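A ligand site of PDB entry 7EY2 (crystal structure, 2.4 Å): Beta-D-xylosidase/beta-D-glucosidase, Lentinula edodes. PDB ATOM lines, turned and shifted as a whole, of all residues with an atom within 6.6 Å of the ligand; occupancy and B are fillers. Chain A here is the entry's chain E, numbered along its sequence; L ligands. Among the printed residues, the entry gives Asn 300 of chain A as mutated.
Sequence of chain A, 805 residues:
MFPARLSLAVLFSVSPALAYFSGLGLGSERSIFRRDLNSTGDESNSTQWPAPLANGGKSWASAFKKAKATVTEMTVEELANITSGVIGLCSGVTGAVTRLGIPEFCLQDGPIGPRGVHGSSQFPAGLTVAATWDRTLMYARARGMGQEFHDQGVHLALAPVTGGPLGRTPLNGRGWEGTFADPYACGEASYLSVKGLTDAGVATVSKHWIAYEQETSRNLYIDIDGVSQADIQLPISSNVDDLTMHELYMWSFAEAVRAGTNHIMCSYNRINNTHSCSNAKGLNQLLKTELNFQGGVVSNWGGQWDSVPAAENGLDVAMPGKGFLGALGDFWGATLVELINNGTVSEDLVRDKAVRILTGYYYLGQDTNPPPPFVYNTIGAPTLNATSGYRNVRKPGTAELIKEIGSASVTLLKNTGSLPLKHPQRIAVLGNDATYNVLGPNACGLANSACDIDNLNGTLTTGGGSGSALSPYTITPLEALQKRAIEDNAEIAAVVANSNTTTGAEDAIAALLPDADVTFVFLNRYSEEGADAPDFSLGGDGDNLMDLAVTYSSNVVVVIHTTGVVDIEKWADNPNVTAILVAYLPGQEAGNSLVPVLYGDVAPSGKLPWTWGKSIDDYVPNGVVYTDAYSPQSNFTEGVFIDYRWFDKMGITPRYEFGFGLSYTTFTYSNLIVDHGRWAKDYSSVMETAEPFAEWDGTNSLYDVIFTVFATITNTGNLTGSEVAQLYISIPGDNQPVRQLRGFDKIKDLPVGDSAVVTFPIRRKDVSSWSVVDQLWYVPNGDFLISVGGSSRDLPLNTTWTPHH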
ATOM      1  N   SER A  91      -4.126 -24.596  25.770  1.00  0.00           N
ATOM      2  CA  SER A  91      -3.157 -23.814  24.948  1.00  0.00           C
ATOM      3  C   SER A  91      -3.500 -22.347  25.113  1.00  0.00           C
ATOM      4  O   SER A  91      -2.640 -21.519  25.225  1.00  0.00           O
ATOM      5  CB  SER A  91      -3.218 -24.176  23.422  1.00  0.00           C
ATOM      6  OG  SER A  91      -3.223 -25.575  23.113  1.00  0.00           O
ATOM      7  N   GLN A 108      -7.493 -25.282  21.952  1.00  0.00           N
ATOM      8  CA  GLN A 108      -6.554 -26.407  22.105  1.00  0.00           C
ATOM      9  C   GLN A 108      -6.027 -26.945  20.812  1.00  0.00           C
ATOM     10  O   GLN A 108      -6.771 -27.287  19.869  1.00  0.00           O
ATOM     11  CB  GLN A 108      -7.251 -27.535  22.858  1.00  0.00           C
ATOM     12  CG  GLN A 108      -6.308 -28.532  23.481  1.00  0.00           C
ATOM     13  CD  GLN A 108      -5.400 -27.914  24.513  1.00  0.00           C
ATOM     14  OE1 GLN A 108      -5.760 -26.922  25.150  1.00  0.00           O
ATOM     15  NE2 GLN A 108      -4.235 -28.464  24.675  1.00  0.00           N
ATOM     16  N   ASP A 109      -4.701 -27.077  20.786  1.00  0.00           N
ATOM     17  CA  ASP A 109      -4.045 -27.830  19.725  1.00  0.00           C
ATOM     18  C   ASP A 109      -4.477 -29.315  19.773  1.00  0.00           C
ATOM     19  O   ASP A 109      -4.806 -29.829  20.858  1.00  0.00           O
ATOM     20  CB  ASP A 109      -2.532 -27.806  19.960  1.00  0.00           C
ATOM     21  CG  ASP A 109      -1.877 -26.460  19.641  1.00  0.00           C
ATOM     22  OD1 ASP A 109      -2.145 -25.878  18.539  1.00  0.00           O
ATOM     23  OD2 ASP A 109      -1.028 -26.049  20.475  1.00  0.00           O
ATOM     24  N   GLY A 110      -4.456 -30.019  18.650  1.00  0.00           N
ATOM     25  CA  GLY A 110      -4.005 -29.480  17.335  1.00  0.00           C
ATOM     26  C   GLY A 110      -4.421 -30.387  16.180  1.00  0.00           C
ATOM     27  O   GLY A 110      -5.291 -31.235  16.353  1.00  0.00           O
ATOM     28  N   PRO A 111      -3.770 -30.248  15.010  1.00  0.00           N
ATOM     29  CA  PRO A 111      -4.277 -30.960  13.832  1.00  0.00           C
ATOM     30  C   PRO A 111      -4.244 -32.504  13.735  1.00  0.00           C
ATOM     31  O   PRO A 111      -4.722 -33.003  12.768  1.00  0.00           O
ATOM     32  CB  PRO A 111      -3.568 -30.295  12.647  1.00  0.00           C
ATOM     33  CG  PRO A 111      -3.081 -28.992  13.193  1.00  0.00           C
ATOM     34  CD  PRO A 111      -2.779 -29.236  14.633  1.00  0.00           C
ATOM     35  N   ARG A 115      -3.704 -32.207  21.926  1.00  0.00           N
ATOM     36  CA  ARG A 115      -2.323 -32.342  22.358  1.00  0.00           C
ATOM     37  C   ARG A 115      -2.198 -32.116  23.889  1.00  0.00           C
ATOM     38  O   ARG A 115      -2.845 -31.288  24.432  1.00  0.00           O
ATOM     39  CB  ARG A 115      -1.445 -31.345  21.603  1.00  0.00           C
ATOM     40  CG  ARG A 115       0.056 -31.532  21.836  1.00  0.00           C
ATOM     41  CD  ARG A 115       0.902 -30.558  21.026  1.00  0.00           C
ATOM     42  NE  ARG A 115       0.539 -29.141  21.256  1.00  0.00           N
ATOM     43  CZ  ARG A 115       1.009 -28.387  22.226  1.00  0.00           C
ATOM     44  NH1 ARG A 115       1.858 -28.869  23.129  1.00  0.00           N
ATOM     45  NH2 ARG A 115       0.583 -27.134  22.309  1.00  0.00           N
ATOM     46  N   LEU A 158      -7.520 -26.029  17.481  1.00  0.00           N
ATOM     47  CA  LEU A 158      -6.600 -25.269  16.637  1.00  0.00           C
ATOM     48  C   LEU A 158      -6.200 -26.230  15.548  1.00  0.00           C
ATOM     49  O   LEU A 158      -5.123 -26.819  15.542  1.00  0.00           O
ATOM     50  CB  LEU A 158      -5.434 -24.712  17.441  1.00  0.00           C
ATOM     51  CG  LEU A 158      -5.927 -23.958  18.692  1.00  0.00           C
ATOM     52  CD1 LEU A 158      -4.799 -23.569  19.648  1.00  0.00           C
ATOM     53  CD2 LEU A 158      -6.788 -22.726  18.332  1.00  0.00           C
ATOM     54  N   ALA A 159      -7.138 -26.386  14.627  1.00  0.00           N
ATOM     55  CA  ALA A 159      -7.090 -27.415  13.581  1.00  0.00           C
ATOM     56  C   ALA A 159      -8.236 -27.130  12.646  1.00  0.00           C
ATOM     57  O   ALA A 159      -9.211 -26.538  13.071  1.00  0.00           O
ATOM     58  CB  ALA A 159      -7.289 -28.770  14.178  1.00  0.00           C
ATOM     59  N   ARG A 174       7.068 -28.218   9.365  1.00  0.00           N
ATOM     60  CA  ARG A 174       5.703 -28.639   9.667  1.00  0.00           C
ATOM     61  C   ARG A 174       4.763 -28.815   8.454  1.00  0.00           C
ATOM     62  O   ARG A 174       3.550 -28.762   8.617  1.00  0.00           O
ATOM     63  CB  ARG A 174       5.085 -27.668  10.716  1.00  0.00           C
ATOM     64  CG  ARG A 174       4.598 -26.361  10.169  1.00  0.00           C
ATOM     65  CD  ARG A 174       4.426 -25.288  11.221  1.00  0.00           C
ATOM     66  NE  ARG A 174       3.396 -25.566  12.178  1.00  0.00           N
ATOM     67  CZ  ARG A 174       2.963 -24.708  13.103  1.00  0.00           C
ATOM     68  NH1 ARG A 174       3.426 -23.466  13.179  1.00  0.00           N
ATOM     69  NH2 ARG A 174       2.016 -25.100  13.940  1.00  0.00           N
ATOM     70  N   GLU A 177       1.816 -31.450   8.781  1.00  0.00           N
ATOM     71  CA  GLU A 177       0.608 -31.166   9.523  1.00  0.00           C
ATOM     72  C   GLU A 177      -0.562 -30.918   8.552  1.00  0.00           C
ATOM     73  O   GLU A 177      -1.708 -31.083   8.926  1.00  0.00           O
ATOM     74  CB  GLU A 177       0.759 -29.952  10.423  1.00  0.00           C
ATOM     75  CG  GLU A 177       1.710 -30.060  11.593  1.00  0.00           C
ATOM     76  CD  GLU A 177       1.579 -28.849  12.544  1.00  0.00           C
ATOM     77  OE1 GLU A 177       2.499 -27.974  12.657  1.00  0.00           O
ATOM     78  OE2 GLU A 177       0.534 -28.751  13.208  1.00  0.00           O
ATOM     79  N   LYS A 207      -5.993 -22.972   9.855  1.00  0.00           N
ATOM     80  CA  LYS A 207      -4.724 -22.267   9.912  1.00  0.00           C
ATOM     81  C   LYS A 207      -3.746 -22.711   8.875  1.00  0.00           C
ATOM     82  O   LYS A 207      -3.944 -23.744   8.259  1.00  0.00           O
ATOM     83  CB  LYS A 207      -4.125 -22.474  11.277  1.00  0.00           C
ATOM     84  CG  LYS A 207      -3.819 -23.899  11.632  1.00  0.00           C
ATOM     85  CD  LYS A 207      -3.670 -24.056  13.122  1.00  0.00           C
ATOM     86  CE  LYS A 207      -2.684 -25.191  13.409  1.00  0.00           C
ATOM     87  NZ  LYS A 207      -2.498 -25.476  14.847  1.00  0.00           N
ATOM     88  N   HIS A 208      -2.684 -21.953   8.616  1.00  0.00           N
ATOM     89  CA  HIS A 208      -2.420 -20.575   9.060  1.00  0.00           C
ATOM     90  C   HIS A 208      -2.527 -19.635   7.853  1.00  0.00           C
ATOM     91  O   HIS A 208      -1.848 -19.836   6.841  1.00  0.00           O
ATOM     92  CB  HIS A 208      -1.004 -20.465   9.610  1.00  0.00           C
ATOM     93  CG  HIS A 208      -0.685 -21.467  10.667  1.00  0.00           C
ATOM     94  ND1 HIS A 208      -0.222 -22.750  10.378  1.00  0.00           N
ATOM     95  CD2 HIS A 208      -0.756 -21.385  12.009  1.00  0.00           C
ATOM     96  CE1 HIS A 208       0.007 -23.388  11.507  1.00  0.00           C
ATOM     97  NE2 HIS A 208      -0.322 -22.589  12.510  1.00  0.00           N
ATOM     98  N   TYR A 212       2.356 -18.845   4.726  1.00  0.00           N
ATOM     99  CA  TYR A 212       3.271 -19.242   5.789  1.00  0.00           C
ATOM    100  C   TYR A 212       4.007 -20.480   5.277  1.00  0.00           C
ATOM    101  O   TYR A 212       3.558 -21.595   5.488  1.00  0.00           O
ATOM    102  CB  TYR A 212       2.458 -19.556   7.069  1.00  0.00           C
ATOM    103  CG  TYR A 212       3.175 -20.139   8.278  1.00  0.00           C
ATOM    104  CD1 TYR A 212       4.356 -19.604   8.747  1.00  0.00           C
ATOM    105  CD2 TYR A 212       2.614 -21.175   8.978  1.00  0.00           C
ATOM    106  CE1 TYR A 212       4.993 -20.144   9.855  1.00  0.00           C
ATOM    107  CE2 TYR A 212       3.226 -21.722  10.110  1.00  0.00           C
ATOM    108  CZ  TYR A 212       4.419 -21.198  10.537  1.00  0.00           C
ATOM    109  OH  TYR A 212       5.013 -21.735  11.661  1.00  0.00           O
ATOM    110  N   GLU A 215       9.556 -22.191   8.087  1.00  0.00           N
ATOM    111  CA  GLU A 215       9.631 -22.038   9.547  1.00  0.00           C
ATOM    112  C   GLU A 215      10.712 -21.104   9.947  1.00  0.00           C
ATOM    113  O   GLU A 215      10.562 -20.384  10.887  1.00  0.00           O
ATOM    114  CB  GLU A 215       9.882 -23.409  10.231  1.00  0.00           C
ATOM    115  CG  GLU A 215       8.682 -24.316  10.231  1.00  0.00           C
ATOM    116  CD  GLU A 215       7.509 -23.675  10.967  1.00  0.00           C
ATOM    117  OE1 GLU A 215       7.522 -23.714  12.230  1.00  0.00           O
ATOM    118  OE2 GLU A 215       6.608 -23.129  10.282  1.00  0.00           O
ATOM    119  N   ARG A 218      10.503 -17.256  11.160  1.00  0.00           N
ATOM    120  CA  ARG A 218       9.066 -16.975  11.379  1.00  0.00           C
ATOM    121  C   ARG A 218       8.904 -15.974  12.544  1.00  0.00           C
ATOM    122  O   ARG A 218       7.966 -15.219  12.555  1.00  0.00           O
ATOM    123  CB  ARG A 218       8.302 -18.302  11.653  1.00  0.00           C
ATOM    124  CG  ARG A 218       8.606 -18.957  12.995  1.00  0.00           C
ATOM    125  CD  ARG A 218       7.882 -20.286  13.141  1.00  0.00           C
ATOM    126  NE  ARG A 218       8.032 -20.787  14.500  1.00  0.00           N
ATOM    127  CZ  ARG A 218       7.182 -21.620  15.125  1.00  0.00           C
ATOM    128  NH1 ARG A 218       6.086 -22.099  14.540  1.00  0.00           N
ATOM    129  NH2 ARG A 218       7.428 -21.982  16.364  1.00  0.00           N
ATOM    130  N   LEU A 220       8.413 -15.511  16.250  1.00  0.00           N
ATOM    131  CA  LEU A 220       7.287 -15.219  17.151  1.00  0.00           C
ATOM    132  C   LEU A 220       7.673 -13.964  17.915  1.00  0.00           C
ATOM    133  O   LEU A 220       8.856 -13.780  18.203  1.00  0.00           O
ATOM    134  CB  LEU A 220       7.004 -16.310  18.197  1.00  0.00           C
ATOM    135  CG  LEU A 220       7.343 -17.793  18.074  1.00  0.00           C
ATOM    136  CD1 LEU A 220       6.647 -18.586  19.190  1.00  0.00           C
ATOM    137  CD2 LEU A 220       7.008 -18.379  16.705  1.00  0.00           C
ATOM    138  N   MET A 265      -6.931 -18.752  11.849  1.00  0.00           N
ATOM    139  CA  MET A 265      -5.721 -18.277  12.538  1.00  0.00           C
ATOM    140  C   MET A 265      -4.868 -17.506  11.571  1.00  0.00           C
ATOM    141  O   MET A 265      -4.629 -18.013  10.502  1.00  0.00           O
ATOM    142  CB  MET A 265      -4.884 -19.452  13.091  1.00  0.00           C
ATOM    143  CG  MET A 265      -3.812 -18.998  14.054  1.00  0.00           C
ATOM    144  SD  MET A 265      -3.029 -20.253  15.072  1.00  0.00           S
ATOM    145  CE  MET A 265      -4.294 -20.478  16.303  1.00  0.00           C
ATOM    146  N   TYR A 268       2.540 -16.253  11.300  1.00  0.00           N
ATOM    147  CA  TYR A 268       3.719 -15.587  11.816  1.00  0.00           C
ATOM    148  C   TYR A 268       4.432 -14.687  10.825  1.00  0.00           C
ATOM    149  O   TYR A 268       5.035 -13.694  11.181  1.00  0.00           O
ATOM    150  CB  TYR A 268       4.747 -16.602  12.376  1.00  0.00           C
ATOM    151  CG  TYR A 268       4.355 -17.263  13.687  1.00  0.00           C
ATOM    152  CD1 TYR A 268       4.041 -16.505  14.800  1.00  0.00           C
ATOM    153  CD2 TYR A 268       4.346 -18.668  13.824  1.00  0.00           C
ATOM    154  CE1 TYR A 268       3.705 -17.126  16.021  1.00  0.00           C
ATOM    155  CE2 TYR A 268       4.007 -19.290  15.025  1.00  0.00           C
ATOM    156  CZ  TYR A 268       3.693 -18.532  16.138  1.00  0.00           C
ATOM    157  OH  TYR A 268       3.326 -19.140  17.332  1.00  0.00           O
ATOM    158  N   SER A 299      -5.131 -14.794  16.639  1.00  0.00           N
ATOM    159  CA  SER A 299      -3.689 -14.609  16.435  1.00  0.00           C
ATOM    160  C   SER A 299      -2.962 -15.931  16.674  1.00  0.00           C
ATOM    161  O   SER A 299      -3.374 -16.711  17.527  1.00  0.00           O
ATOM    162  CB  SER A 299      -3.114 -13.588  17.441  1.00  0.00           C
ATOM    163  OG  SER A 299      -3.034 -14.161  18.742  1.00  0.00           O
ATOM    164  N   ASN A 300      -1.869 -16.161  15.968  1.00  0.00           N
ATOM    165  CA  ASN A 300      -0.890 -17.152  16.393  1.00  0.00           C
ATOM    166  C   ASN A 300      -0.382 -16.752  17.753  1.00  0.00           C
ATOM    167  O   ASN A 300      -0.471 -15.602  18.134  1.00  0.00           O
ATOM    168  CB  ASN A 300       0.314 -17.148  15.461  1.00  0.00           C
ATOM    169  CG  ASN A 300       0.255 -18.230  14.442  1.00  0.00           C
ATOM    170  OD1 ASN A 300      -0.140 -17.958  13.318  1.00  0.00           O
ATOM    171  ND2 ASN A 300       0.678 -19.488  14.815  1.00  0.00           N
ATOM    172  N   TRP A 301       0.200 -17.716  18.467  1.00  0.00           N
ATOM    173  CA  TRP A 301       0.782 -17.441  19.770  1.00  0.00           C
ATOM    174  C   TRP A 301       2.079 -16.665  19.568  1.00  0.00           C
ATOM    175  O   TRP A 301       3.055 -17.227  19.111  1.00  0.00           O
ATOM    176  CB  TRP A 301       1.006 -18.769  20.507  1.00  0.00           C
ATOM    177  CG  TRP A 301      -0.209 -19.379  21.268  1.00  0.00           C
ATOM    178  CD1 TRP A 301      -0.158 -19.901  22.480  1.00  0.00           C
ATOM    179  CD2 TRP A 301      -1.587 -19.494  20.864  1.00  0.00           C
ATOM    180  NE1 TRP A 301      -1.351 -20.383  22.860  1.00  0.00           N
ATOM    181  CE2 TRP A 301      -2.263 -20.147  21.893  1.00  0.00           C
ATOM    182  CE3 TRP A 301      -2.313 -19.186  19.696  1.00  0.00           C
ATOM    183  CZ2 TRP A 301      -3.622 -20.474  21.837  1.00  0.00           C
ATOM    184  CZ3 TRP A 301      -3.666 -19.504  19.639  1.00  0.00           C
ATOM    185  CH2 TRP A 301      -4.307 -20.140  20.692  1.00  0.00           C
ATOM    186  N   GLY A 302       2.082 -15.370  19.860  1.00  0.00           N
ATOM    187  CA  GLY A 302       3.169 -14.469  19.452  1.00  0.00           C
ATOM    188  C   GLY A 302       3.069 -14.004  18.006  1.00  0.00           C
ATOM    189  O   GLY A 302       4.027 -13.523  17.407  1.00  0.00           O
ATOM    190  N   GLY A 465       6.118 -30.565  17.553  1.00  0.00           N
ATOM    191  CA  GLY A 465       5.594 -29.203  17.747  1.00  0.00           C
ATOM    192  C   GLY A 465       4.147 -29.230  18.220  1.00  0.00           C
ATOM    193  O   GLY A 465       3.644 -30.254  18.699  1.00  0.00           O
ATOM    194  N   SER A 466       3.441 -28.138  17.974  1.00  0.00           N
ATOM    195  CA  SER A 466       2.081 -27.940  18.428  1.00  0.00           C
ATOM    196  C   SER A 466       1.061 -28.905  17.837  1.00  0.00           C
ATOM    197  O   SER A 466      -0.044 -29.038  18.396  1.00  0.00           O
ATOM    198  CB  SER A 466       1.646 -26.494  18.152  1.00  0.00           C
ATOM    199  OG  SER A 466       1.951 -26.176  16.824  1.00  0.00           O
ATOM    200  N   GLU A 529       7.992 -28.158  13.930  1.00  0.00           N
ATOM    201  CA  GLU A 529       7.764 -26.721  13.867  1.00  0.00           C
ATOM    202  C   GLU A 529       8.972 -26.002  14.479  1.00  0.00           C
ATOM    203  O   GLU A 529       9.666 -26.552  15.356  1.00  0.00           O
ATOM    204  CB  GLU A 529       6.446 -26.306  14.530  1.00  0.00           C
ATOM    205  CG  GLU A 529       6.581 -25.914  15.974  1.00  0.00           C
ATOM    206  CD  GLU A 529       5.350 -25.206  16.504  1.00  0.00           C
ATOM    207  OE1 GLU A 529       4.266 -25.822  16.609  1.00  0.00           O
ATOM    208  OE2 GLU A 529       5.493 -24.018  16.819  1.00  0.00           O
HETATM  209  C1  LIG L   1       2.743 -22.710  16.539  1.00  0.00           C
HETATM  210  C2  LIG L   1       1.207 -22.891  16.625  1.00  0.00           C
HETATM  211  C3  LIG L   1       0.747 -22.097  17.880  1.00  0.00           C
HETATM  212  C4  LIG L   1      -0.623 -22.420  18.533  1.00  0.00           C
HETATM  213  C5  LIG L   1      -1.741 -22.569  17.517  1.00  0.00           C
HETATM  214  O1  LIG L   1       3.334 -22.999  17.837  1.00  0.00           O
HETATM  215  O2  LIG L   1       0.448 -22.527  15.399  1.00  0.00           O
HETATM  216  O3  LIG L   1       0.753 -20.748  17.422  1.00  0.00           O
HETATM  217  O4  LIG L   1      -0.663 -23.541  19.454  1.00  0.00           O
HETATM  218  O5  LIG L   1      -1.587 -23.627  16.628  1.00  0.00           O
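A ring nitrogen (NE2) of His 208 is in hydrogen-bond range of an oxygen (O2) of the ligand (3.0 Å).
The side-chain carboxylate (OE2) of Glu 529 is in hydrogen-bond range of an oxygen (O1) of the ligand (2.6 Å).
O3 of the ligand is in hydrogen-bond range of OH of Tyr 268 (3.0 Å).
NZ of Lys 207 sits at hydrogen-bond distance from O5 of the ligand (2.7 Å).
The side-chain amide nitrogen of Asn 300 is in hydrogen-bond range of an oxygen (O3) of the ligand (2.9 Å).
NH2 of Arg 174 is in hydrogen-bond range of O2 of the ligand, 3.3 Å away.
An oxygen (O3) of the ligand is in hydrogen-bond range of the backbone NH (N) of Trp 301, at 3.3 Å.
OD2 of Asp 109 sits at hydrogen-bond distance from O4 of the ligand.
NE of Arg 115 lies within hydrogen-bond range of O of Ser 466, 2.9 Å away.
The backbone carbonyl oxygen (O) of Ser 91 is in hydrogen-bond range of the indole nitrogen (NE1) of Trp 301 (2.9 Å).
The guanidinium group of Arg 174 is in hydrogen-bond range of the side-chain hydroxyl of Tyr 212.
The side-chain hydroxyl (OG) of Ser 91 sits at hydrogen-bond distance from the backbone NH (N) of Asp 109.
OD1 of Asp 109 is in salt-bridge range of NZ of Lys 207, at 3.7 Å.
The guanidinium group (NH1) of Arg 218 is in hydrogen-bond range of the side-chain hydroxyl (OH) of Tyr 212 (3.1 Å).
NZ of Lys 207 is in hydrogen-bond range of O of Leu 158, 3.0 Å away.
The guanidinium group (NH2) of Arg 174 is in hydrogen-bond range of the side-chain hydroxyl (OG) of Ser 466, at 3.1 Å.
Merely in contact with the ligand: Leu 158 (3.9 Å), Arg 218 (3.9 Å), Met 265 (3.5 Å) and Ser 466 (3.4 Å).
Hydrophobic or aromatic side chains that line the ligand: Leu 158, His 208, Met 265, Tyr 268 and Trp 301.
Within 4 Å of the ligand: Asp 109, Leu 158, Arg 174, Lys 207, His 208, Arg 218, Met 265, Tyr 268, Asn 300, Trp 301, Ser 466 and Glu 529.
The nearest printed residue that does not touch the ligand is Arg 115 (4.8 Å).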
